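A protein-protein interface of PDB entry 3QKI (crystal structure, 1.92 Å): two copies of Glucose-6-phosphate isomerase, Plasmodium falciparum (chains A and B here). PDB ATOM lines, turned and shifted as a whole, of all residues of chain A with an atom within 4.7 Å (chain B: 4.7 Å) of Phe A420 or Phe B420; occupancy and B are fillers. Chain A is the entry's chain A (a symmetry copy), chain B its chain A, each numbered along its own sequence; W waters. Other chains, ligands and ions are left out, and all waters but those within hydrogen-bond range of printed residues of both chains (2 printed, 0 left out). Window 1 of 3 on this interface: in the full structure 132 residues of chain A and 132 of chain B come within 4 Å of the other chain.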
ATOM      1  N   ASN A 375      24.398  18.289  11.130  1.00  0.00           N
ATOM      2  CA  ASN A 375      23.942  18.719  12.451  1.00  0.00           C
ATOM      3  C   ASN A 375      24.604  20.015  12.848  1.00  0.00           C
ATOM      4  O   ASN A 375      25.683  20.320  12.349  1.00  0.00           O
ATOM      5  CB  ASN A 375      24.265  17.659  13.516  1.00  0.00           C
ATOM      6  CG  ASN A 375      23.504  16.398  13.373  1.00  0.00           C
ATOM      7  OD1 ASN A 375      22.373  16.276  13.805  1.00  0.00           O
ATOM      8  ND2 ASN A 375      24.109  15.436  12.738  1.00  0.00           N
ATOM      9  N   VAL A 376      23.960  20.776  13.754  1.00  0.00           N
ATOM     10  CA  VAL A 376      24.510  21.996  14.346  1.00  0.00           C
ATOM     11  C   VAL A 376      24.155  21.917  15.825  1.00  0.00           C
ATOM     12  O   VAL A 376      22.972  21.757  16.157  1.00  0.00           O
ATOM     13  CB  VAL A 376      23.970  23.336  13.742  1.00  0.00           C
ATOM     14  CG1 VAL A 376      24.488  24.544  14.535  1.00  0.00           C
ATOM     15  CG2 VAL A 376      24.295  23.477  12.260  1.00  0.00           C
ATOM     16  N   ALA A 377      25.153  22.063  16.709  1.00  0.00           N
ATOM     17  CA  ALA A 377      24.930  22.133  18.162  1.00  0.00           C
ATOM     18  C   ALA A 377      24.993  23.608  18.586  1.00  0.00           C
ATOM     19  O   ALA A 377      26.006  24.278  18.343  1.00  0.00           O
ATOM     20  CB  ALA A 377      25.970  21.306  18.916  1.00  0.00           C
ATOM     21  N   ILE A 378      23.898  24.115  19.186  1.00  0.00           N
ATOM     22  CA  ILE A 378      23.785  25.499  19.671  1.00  0.00           C
ATOM     23  C   ILE A 378      24.068  25.430  21.131  1.00  0.00           C
ATOM     24  O   ILE A 378      23.276  24.861  21.895  1.00  0.00           O
ATOM     25  CB  ILE A 378      22.407  26.132  19.387  1.00  0.00           C
ATOM     26  CG1 ILE A 378      22.103  26.189  17.871  1.00  0.00           C
ATOM     27  CG2 ILE A 378      22.304  27.532  20.046  1.00  0.00           C
ATOM     28  CD1 ILE A 378      23.074  27.117  16.933  1.00  0.00           C
ATOM     29  N   SER A 389      18.137  27.670  22.112  1.00  0.00           N
ATOM     30  CA  SER A 389      18.227  26.490  21.222  1.00  0.00           C
ATOM     31  C   SER A 389      16.846  26.046  20.699  1.00  0.00           C
ATOM     32  O   SER A 389      16.724  25.754  19.505  1.00  0.00           O
ATOM     33  CB  SER A 389      18.880  25.333  21.983  1.00  0.00           C
ATOM     34  OG  SER A 389      18.991  24.148  21.223  1.00  0.00           O
ATOM     35  N   GLN A 393      15.912  26.066  16.823  1.00  0.00           N
ATOM     36  CA  GLN A 393      15.410  24.826  16.203  1.00  0.00           C
ATOM     37  C   GLN A 393      14.266  25.088  15.260  1.00  0.00           C
ATOM     38  O   GLN A 393      14.345  24.641  14.120  1.00  0.00           O
ATOM     39  CB  GLN A 393      14.934  23.844  17.269  1.00  0.00           C
ATOM     40  CG  GLN A 393      15.924  22.815  17.594  1.00  0.00           C
ATOM     41  CD  GLN A 393      15.336  21.794  18.541  1.00  0.00           C
ATOM     42  OE1 GLN A 393      14.274  21.987  19.152  1.00  0.00           O
ATOM     43  NE2 GLN A 393      16.022  20.673  18.668  1.00  0.00           N
ATOM     44  N   MET A 397      15.041  24.959  11.308  1.00  0.00           N
ATOM     45  CA  MET A 397      14.450  23.751  10.766  1.00  0.00           C
ATOM     46  C   MET A 397      13.157  23.929  10.004  1.00  0.00           C
ATOM     47  O   MET A 397      12.965  23.275   8.978  1.00  0.00           O
ATOM     48  CB  MET A 397      14.361  22.656  11.831  1.00  0.00           C
ATOM     49  CG  MET A 397      15.739  22.259  12.349  1.00  0.00           C
ATOM     50  SD  MET A 397      15.762  21.152  13.742  1.00  0.00           S
ATOM     51  CE  MET A 397      15.285  19.582  12.978  1.00  0.00           C
ATOM     52  N   VAL A 418      20.063  19.289  11.418  1.00  0.00           N
ATOM     53  CA  VAL A 418      19.300  19.041  12.642  1.00  0.00           C
ATOM     54  C   VAL A 418      19.984  19.944  13.689  1.00  0.00           C
ATOM     55  O   VAL A 418      21.194  19.865  13.872  1.00  0.00           O
ATOM     56  CB  VAL A 418      19.339  17.568  13.086  1.00  0.00           C
ATOM     57  CG1 VAL A 418      18.862  17.433  14.519  1.00  0.00           C
ATOM     58  CG2 VAL A 418      18.500  16.699  12.161  1.00  0.00           C
ATOM     59  N   TYR A 419      19.216  20.824  14.330  1.00  0.00           N
ATOM     60  CA  TYR A 419      19.728  21.712  15.371  1.00  0.00           C
ATOM     61  C   TYR A 419      19.340  21.152  16.721  1.00  0.00           C
ATOM     62  O   TYR A 419      18.214  20.673  16.901  1.00  0.00           O
ATOM     63  CB  TYR A 419      19.123  23.111  15.225  1.00  0.00           C
ATOM     64  CG  TYR A 419      19.825  23.990  14.234  1.00  0.00           C
ATOM     65  CD1 TYR A 419      20.587  25.073  14.656  1.00  0.00           C
ATOM     66  CD2 TYR A 419      19.708  23.764  12.862  1.00  0.00           C
ATOM     67  CE1 TYR A 419      21.207  25.922  13.736  1.00  0.00           C
ATOM     68  CE2 TYR A 419      20.377  24.568  11.937  1.00  0.00           C
ATOM     69  CZ  TYR A 419      21.101  25.662  12.378  1.00  0.00           C
ATOM     70  OH  TYR A 419      21.713  26.489  11.464  1.00  0.00           O
ATOM     71  N   PHE A 420      20.270  21.220  17.679  1.00  0.00           N
ATOM     72  CA  PHE A 420      20.020  20.761  19.038  1.00  0.00           C
ATOM     73  C   PHE A 420      21.008  21.464  19.968  1.00  0.00           C
ATOM     74  O   PHE A 420      21.886  22.210  19.513  1.00  0.00           O
ATOM     75  CB  PHE A 420      20.140  19.215  19.136  1.00  0.00           C
ATOM     76  CG  PHE A 420      21.564  18.703  19.135  1.00  0.00           C
ATOM     77  CD1 PHE A 420      22.175  18.283  20.321  1.00  0.00           C
ATOM     78  CD2 PHE A 420      22.316  18.682  17.959  1.00  0.00           C
ATOM     79  CE1 PHE A 420      23.497  17.825  20.321  1.00  0.00           C
ATOM     80  CE2 PHE A 420      23.639  18.234  17.959  1.00  0.00           C
ATOM     81  CZ  PHE A 420      24.217  17.797  19.136  1.00  0.00           C
ATOM     82  N   GLY A 421      20.867  21.220  21.254  1.00  0.00           N
ATOM     83  CA  GLY A 421      21.781  21.790  22.220  1.00  0.00           C
ATOM     84  C   GLY A 421      21.197  22.017  23.586  1.00  0.00           C
ATOM     85  O   GLY A 421      19.979  21.978  23.782  1.00  0.00           O
ATOM     86  N   PHE A 431      26.465  15.243  26.463  1.00  0.00           N
ATOM     87  CA  PHE A 431      26.743  14.616  25.179  1.00  0.00           C
ATOM     88  C   PHE A 431      28.061  15.012  24.475  1.00  0.00           C
ATOM     89  O   PHE A 431      28.259  14.579  23.334  1.00  0.00           O
ATOM     90  CB  PHE A 431      25.550  14.861  24.233  1.00  0.00           C
ATOM     91  CG  PHE A 431      25.180  16.330  24.107  1.00  0.00           C
ATOM     92  CD1 PHE A 431      25.972  17.207  23.360  1.00  0.00           C
ATOM     93  CD2 PHE A 431      24.057  16.840  24.758  1.00  0.00           C
ATOM     94  CE1 PHE A 431      25.671  18.571  23.306  1.00  0.00           C
ATOM     95  CE2 PHE A 431      23.749  18.201  24.688  1.00  0.00           C
ATOM     96  CZ  PHE A 431      24.562  19.061  23.969  1.00  0.00           C
ATOM     97  N   ILE A 435      30.516  14.502  20.601  1.00  0.00           N
ATOM     98  CA  ILE A 435      31.064  15.664  19.873  1.00  0.00           C
ATOM     99  C   ILE A 435      32.590  15.565  19.753  1.00  0.00           C
ATOM    100  O   ILE A 435      33.144  16.003  18.739  1.00  0.00           O
ATOM    101  CB  ILE A 435      30.546  17.024  20.437  1.00  0.00           C
ATOM    102  CG1 ILE A 435      28.993  17.075  20.389  1.00  0.00           C
ATOM    103  CG2 ILE A 435      31.166  18.235  19.690  1.00  0.00           C
ATOM    104  CD1 ILE A 435      28.306  18.442  20.783  1.00  0.00           C
ATOM    105  N   ILE A 441      30.228  16.990  14.785  1.00  0.00           N
ATOM    106  CA  ILE A 441      29.101  17.918  14.927  1.00  0.00           C
ATOM    107  C   ILE A 441      29.613  19.364  15.063  1.00  0.00           C
ATOM    108  O   ILE A 441      30.095  19.728  16.139  1.00  0.00           O
ATOM    109  CB  ILE A 441      28.152  17.521  16.103  1.00  0.00           C
ATOM    110  CG1 ILE A 441      27.476  16.153  15.803  1.00  0.00           C
ATOM    111  CG2 ILE A 441      27.068  18.610  16.332  1.00  0.00           C
ATOM    112  CD1 ILE A 441      27.459  15.397  16.797  1.00  0.00           C
ATOM    113  N   ASN B 375      20.343  10.389  13.012  1.00  0.00           N
ATOM    114  CA  ASN B 375      19.612  11.129  14.040  1.00  0.00           C
ATOM    115  C   ASN B 375      18.473  10.301  14.584  1.00  0.00           C
ATOM    116  O   ASN B 375      17.995   9.405  13.895  1.00  0.00           O
ATOM    117  CB  ASN B 375      19.037  12.437  13.472  1.00  0.00           C
ATOM    118  CG  ASN B 375      20.057  13.442  13.102  1.00  0.00           C
ATOM    119  OD1 ASN B 375      20.554  14.189  13.925  1.00  0.00           O
ATOM    120  ND2 ASN B 375      20.407  13.464  11.848  1.00  0.00           N
ATOM    121  N   VAL B 376      18.034  10.607  15.820  1.00  0.00           N
ATOM    122  CA  VAL B 376      16.865   9.997  16.454  1.00  0.00           C
ATOM    123  C   VAL B 376      16.131  11.149  17.129  1.00  0.00           C
ATOM    124  O   VAL B 376      16.742  11.872  17.928  1.00  0.00           O
ATOM    125  CB  VAL B 376      17.179   8.880  17.505  1.00  0.00           C
ATOM    126  CG1 VAL B 376      15.899   8.421  18.219  1.00  0.00           C
ATOM    127  CG2 VAL B 376      17.914   7.695  16.891  1.00  0.00           C
ATOM    128  N   ALA B 377      14.829  11.301  16.846  1.00  0.00           N
ATOM    129  CA  ALA B 377      13.975  12.292  17.522  1.00  0.00           C
ATOM    130  C   ALA B 377      13.154  11.563  18.598  1.00  0.00           C
ATOM    131  O   ALA B 377      12.425  10.614  18.280  1.00  0.00           O
ATOM    132  CB  ALA B 377      13.059  12.998  16.524  1.00  0.00           C
ATOM    133  N   ILE B 378      13.304  11.987  19.867  1.00  0.00           N
ATOM    134  CA  ILE B 378      12.589  11.418  21.020  1.00  0.00           C
ATOM    135  C   ILE B 378      11.443  12.337  21.266  1.00  0.00           C
ATOM    136  O   ILE B 378      11.642  13.490  21.674  1.00  0.00           O
ATOM    137  CB  ILE B 378      13.477  11.268  22.272  1.00  0.00           C
ATOM    138  CG1 ILE B 378      14.679  10.327  22.014  1.00  0.00           C
ATOM    139  CG2 ILE B 378      12.633  10.800  23.486  1.00  0.00           C
ATOM    140  CD1 ILE B 378      14.358   8.758  21.665  1.00  0.00           C
ATOM    141  N   SER B 389      13.948  13.471  27.062  1.00  0.00           N
ATOM    142  CA  SER B 389      14.882  13.642  25.926  1.00  0.00           C
ATOM    143  C   SER B 389      16.294  14.056  26.389  1.00  0.00           C
ATOM    144  O   SER B 389      17.275  13.502  25.883  1.00  0.00           O
ATOM    145  CB  SER B 389      14.326  14.703  24.973  1.00  0.00           C
ATOM    146  OG  SER B 389      15.161  14.957  23.862  1.00  0.00           O
ATOM    147  N   GLN B 393      19.510  11.788  25.750  1.00  0.00           N
ATOM    148  CA  GLN B 393      20.674  12.377  25.062  1.00  0.00           C
ATOM    149  C   GLN B 393      21.975  11.960  25.693  1.00  0.00           C
ATOM    150  O   GLN B 393      22.839  11.478  24.967  1.00  0.00           O
ATOM    151  CB  GLN B 393      20.599  13.901  25.084  1.00  0.00           C
ATOM    152  CG  GLN B 393      20.073  14.474  23.844  1.00  0.00           C
ATOM    153  CD  GLN B 393      20.166  15.983  23.876  1.00  0.00           C
ATOM    154  OE1 GLN B 393      20.390  16.614  24.919  1.00  0.00           O
ATOM    155  NE2 GLN B 393      20.002  16.589  22.714  1.00  0.00           N
ATOM    156  N   MET B 397      24.165   9.169  23.782  1.00  0.00           N
ATOM    157  CA  MET B 397      25.324   9.819  23.200  1.00  0.00           C
ATOM    158  C   MET B 397      26.630   9.628  23.936  1.00  0.00           C
ATOM    159  O   MET B 397      27.666   9.450  23.293  1.00  0.00           O
ATOM    160  CB  MET B 397      25.033  11.287  22.887  1.00  0.00           C
ATOM    161  CG  MET B 397      23.908  11.435  21.868  1.00  0.00           C
ATOM    162  SD  MET B 397      23.327  13.092  21.579  1.00  0.00           S
ATOM    163  CE  MET B 397      24.681  13.798  20.608  1.00  0.00           C
ATOM    164  N   VAL B 418      22.675  11.362  16.685  1.00  0.00           N
ATOM    165  CA  VAL B 418      22.438  12.593  17.438  1.00  0.00           C
ATOM    166  C   VAL B 418      20.980  12.453  17.923  1.00  0.00           C
ATOM    167  O   VAL B 418      20.085  12.222  17.117  1.00  0.00           O
ATOM    168  CB  VAL B 418      22.607  13.862  16.583  1.00  0.00           C
ATOM    169  CG1 VAL B 418      22.003  15.061  17.288  1.00  0.00           C
ATOM    170  CG2 VAL B 418      24.074  14.114  16.267  1.00  0.00           C
ATOM    171  N   TYR B 419      20.762  12.545  19.233  1.00  0.00           N
ATOM    172  CA  TYR B 419      19.426  12.468  19.821  1.00  0.00           C
ATOM    173  C   TYR B 419      18.962  13.867  20.157  1.00  0.00           C
ATOM    174  O   TYR B 419      19.745  14.684  20.656  1.00  0.00           O
ATOM    175  CB  TYR B 419      19.456  11.636  21.106  1.00  0.00           C
ATOM    176  CG  TYR B 419      19.364  10.155  20.888  1.00  0.00           C
ATOM    177  CD1 TYR B 419      18.215   9.454  21.233  1.00  0.00           C
ATOM    178  CD2 TYR B 419      20.440   9.438  20.365  1.00  0.00           C
ATOM    179  CE1 TYR B 419      18.140   8.068  21.074  1.00  0.00           C
ATOM    180  CE2 TYR B 419      20.351   8.062  20.141  1.00  0.00           C
ATOM    181  CZ  TYR B 419      19.210   7.378  20.524  1.00  0.00           C
ATOM    182  OH  TYR B 419      19.145   6.013  20.359  1.00  0.00           O
ATOM    183  N   PHE B 420      17.681  14.144  19.893  1.00  0.00           N
ATOM    184  CA  PHE B 420      17.086  15.436  20.206  1.00  0.00           C
ATOM    185  C   PHE B 420      15.573  15.249  20.314  1.00  0.00           C
ATOM    186  O   PHE B 420      15.049  14.155  20.067  1.00  0.00           O
ATOM    187  CB  PHE B 420      17.458  16.496  19.133  1.00  0.00           C
ATOM    188  CG  PHE B 420      16.690  16.362  17.837  1.00  0.00           C
ATOM    189  CD1 PHE B 420      15.630  17.224  17.539  1.00  0.00           C
ATOM    190  CD2 PHE B 420      16.992  15.346  16.928  1.00  0.00           C
ATOM    191  CE1 PHE B 420      14.911  17.089  16.346  1.00  0.00           C
ATOM    192  CE2 PHE B 420      16.269  15.203  15.741  1.00  0.00           C
ATOM    193  CZ  PHE B 420      15.242  16.082  15.453  1.00  0.00           C
ATOM    194  N   GLY B 421      14.883  16.312  20.672  1.00  0.00           N
ATOM    195  CA  GLY B 421      13.439  16.264  20.754  1.00  0.00           C
ATOM    196  C   GLY B 421      12.829  17.212  21.748  1.00  0.00           C
ATOM    197  O   GLY B 421      13.515  17.775  22.606  1.00  0.00           O
ATOM    198  N   PHE B 431       9.686  21.894  14.668  1.00  0.00           N
ATOM    199  CA  PHE B 431      10.576  21.370  13.642  1.00  0.00           C
ATOM    200  C   PHE B 431      10.047  20.197  12.786  1.00  0.00           C
ATOM    201  O   PHE B 431      10.829  19.666  11.989  1.00  0.00           O
ATOM    202  CB  PHE B 431      11.918  20.980  14.294  1.00  0.00           C
ATOM    203  CG  PHE B 431      11.754  20.036  15.474  1.00  0.00           C
ATOM    204  CD1 PHE B 431      11.441  18.688  15.276  1.00  0.00           C
ATOM    205  CD2 PHE B 431      11.888  20.500  16.783  1.00  0.00           C
ATOM    206  CE1 PHE B 431      11.219  17.838  16.364  1.00  0.00           C
ATOM    207  CE2 PHE B 431      11.682  19.645  17.868  1.00  0.00           C
ATOM    208  CZ  PHE B 431      11.341  18.320  17.653  1.00  0.00           C
ATOM    209  N   ILE B 435      11.203  17.152   9.517  1.00  0.00           N
ATOM    210  CA  ILE B 435      10.942  15.707   9.677  1.00  0.00           C
ATOM    211  C   ILE B 435      10.049  15.183   8.547  1.00  0.00           C
ATOM    212  O   ILE B 435      10.219  14.033   8.130  1.00  0.00           O
ATOM    213  CB  ILE B 435      10.449  15.343  11.113  1.00  0.00           C
ATOM    214  CG1 ILE B 435      11.489  15.797  12.175  1.00  0.00           C
ATOM    215  CG2 ILE B 435      10.137  13.829  11.252  1.00  0.00           C
ATOM    216  CD1 ILE B 435      11.220  15.372  13.673  1.00  0.00           C
ATOM    217  N   ILE B 441      14.472  11.729   9.438  1.00  0.00           N
ATOM    218  CA  ILE B 441      14.809  11.578  10.857  1.00  0.00           C
ATOM    219  C   ILE B 441      13.896  10.528  11.516  1.00  0.00           C
ATOM    220  O   ILE B 441      12.732  10.835  11.788  1.00  0.00           O
ATOM    221  CB  ILE B 441      14.778  12.941  11.622  1.00  0.00           C
ATOM    222  CG1 ILE B 441      15.884  13.885  11.071  1.00  0.00           C
ATOM    223  CG2 ILE B 441      14.974  12.725  13.147  1.00  0.00           C
ATOM    224  CD1 ILE B 441      15.479  15.056  10.910  1.00  0.00           C
HETATM  225  O   HOH W   1      16.210  18.978  21.255  1.00  0.00           O
HETATM  226  O   HOH W   2      18.706  19.375  22.319  1.00  0.00           O
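The side-chain sulfur (SD) of Met A397 sits at hydrogen-bond distance from the backbone NH (N) of Tyr A419 (3.5 Å). The backbone NH (N) of Ile A378 lies within hydrogen-bond range of the backbone carbonyl oxygen (O) of Phe A420, at 2.8 Å. N of Ile B378 sits at hydrogen-bond distance from O of Phe B420 (2.8 Å). SD of Met B397 lies within hydrogen-bond range of N of Tyr B419, 3.5 Å away. NE2 of Gln B393 lies within hydrogen-bond range of O of Tyr B419 (2.8 Å). The backbone carbonyl oxygen of Val A376 lies within hydrogen-bond range of the backbone NH of Phe A420 (3.1 Å).
Water W1 bridges the backbone NH (N) of Gly B421 (3.0 Å) and the side-chain amide nitrogen (NE2) of Gln A393 (3.1 Å). Water W2 lies within hydrogen-bond range of the backbone NH of Gly A421 (3.0 Å) and the side-chain amide nitrogen of Gln B393 (3.1 Å).
The side-chain amide oxygen of Asn B375 sits close to the side-chain amide oxygen of Asn A375 (2.8 Å).
Of the printed residues of chain B, Phe A420 touches Gln B393, Val B418 and Phe B420. Of the printed residues of chain A, Phe B420 touches Gln A393 (3.7 Å), Val A418 (3.6 Å) and Phe A420 (3.8 Å). Printed residues of chain A within 4 Å of Val B418: Asn A375, Phe A420 and Ile A441. Printed residues of chain A within 4 Å of Gln B393: Phe A420 (3.6 Å) and Phe A431 (3.7 Å). Of the printed residues of chain A, Asn B375 touches Asn A375 and Val A418. Printed residues of chain B within 4 Å of Met A397: Phe B431. Printed residues of chain B within 4 Å of Gln A393: Phe B420 and Phe B431. The nearest residue of chain A that does not touch Phe B420 is Met A397 (4.2 Å).
Asn A375 touches Val B418, and with the chains exchanged Val A418 touches Asn B375. Met A397 touches Phe B431, and with the chains exchanged Phe A431 touches Met B397. Val A418 touches Phe B420, and with the chains exchanged Phe A420 touches Val B418. Phe B420 touches its own counterpart, Phe A420.
Among the printed residues, merely in contact across the chains: Asn A375 with Val B418 (3.7 Å), Gln A393 with Phe B420 (3.7 Å), Gln A393 with Phe B431 (3.7 Å), Met A397 with Phe B431 (3.9 Å), Val A418 with Asn B375 (3.7 Å), Val A418 with Phe B420 (3.6 Å), Val A418 with Ile B441 (3.7 Å), Phe A420 with Gln B393 (3.6 Å), Phe A420 with Val B418 (3.6 Å), Phe A420 with Phe B420 (3.8 Å), Phe A431 with Gln B393 (3.7 Å), Phe A431 with Met B397 (3.9 Å) and Ile A441 with Val B418 (3.7 Å).
Of the 14 printed residues of chain A, 7 touch a printed residue of chain B. Hydrophobic or aromatic side chains of chain B that line the printed part of chain A: Met B397, Val B418, Phe B420, Phe B431 and Ile B441. Along chain B the printed residues that touch a printed residue of chain A span positions 375 to 441. Among the printed residues, no Asp or Glu carboxylate lies within 4 Å of a Lys or Arg side-chain nitrogen of the other chain.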
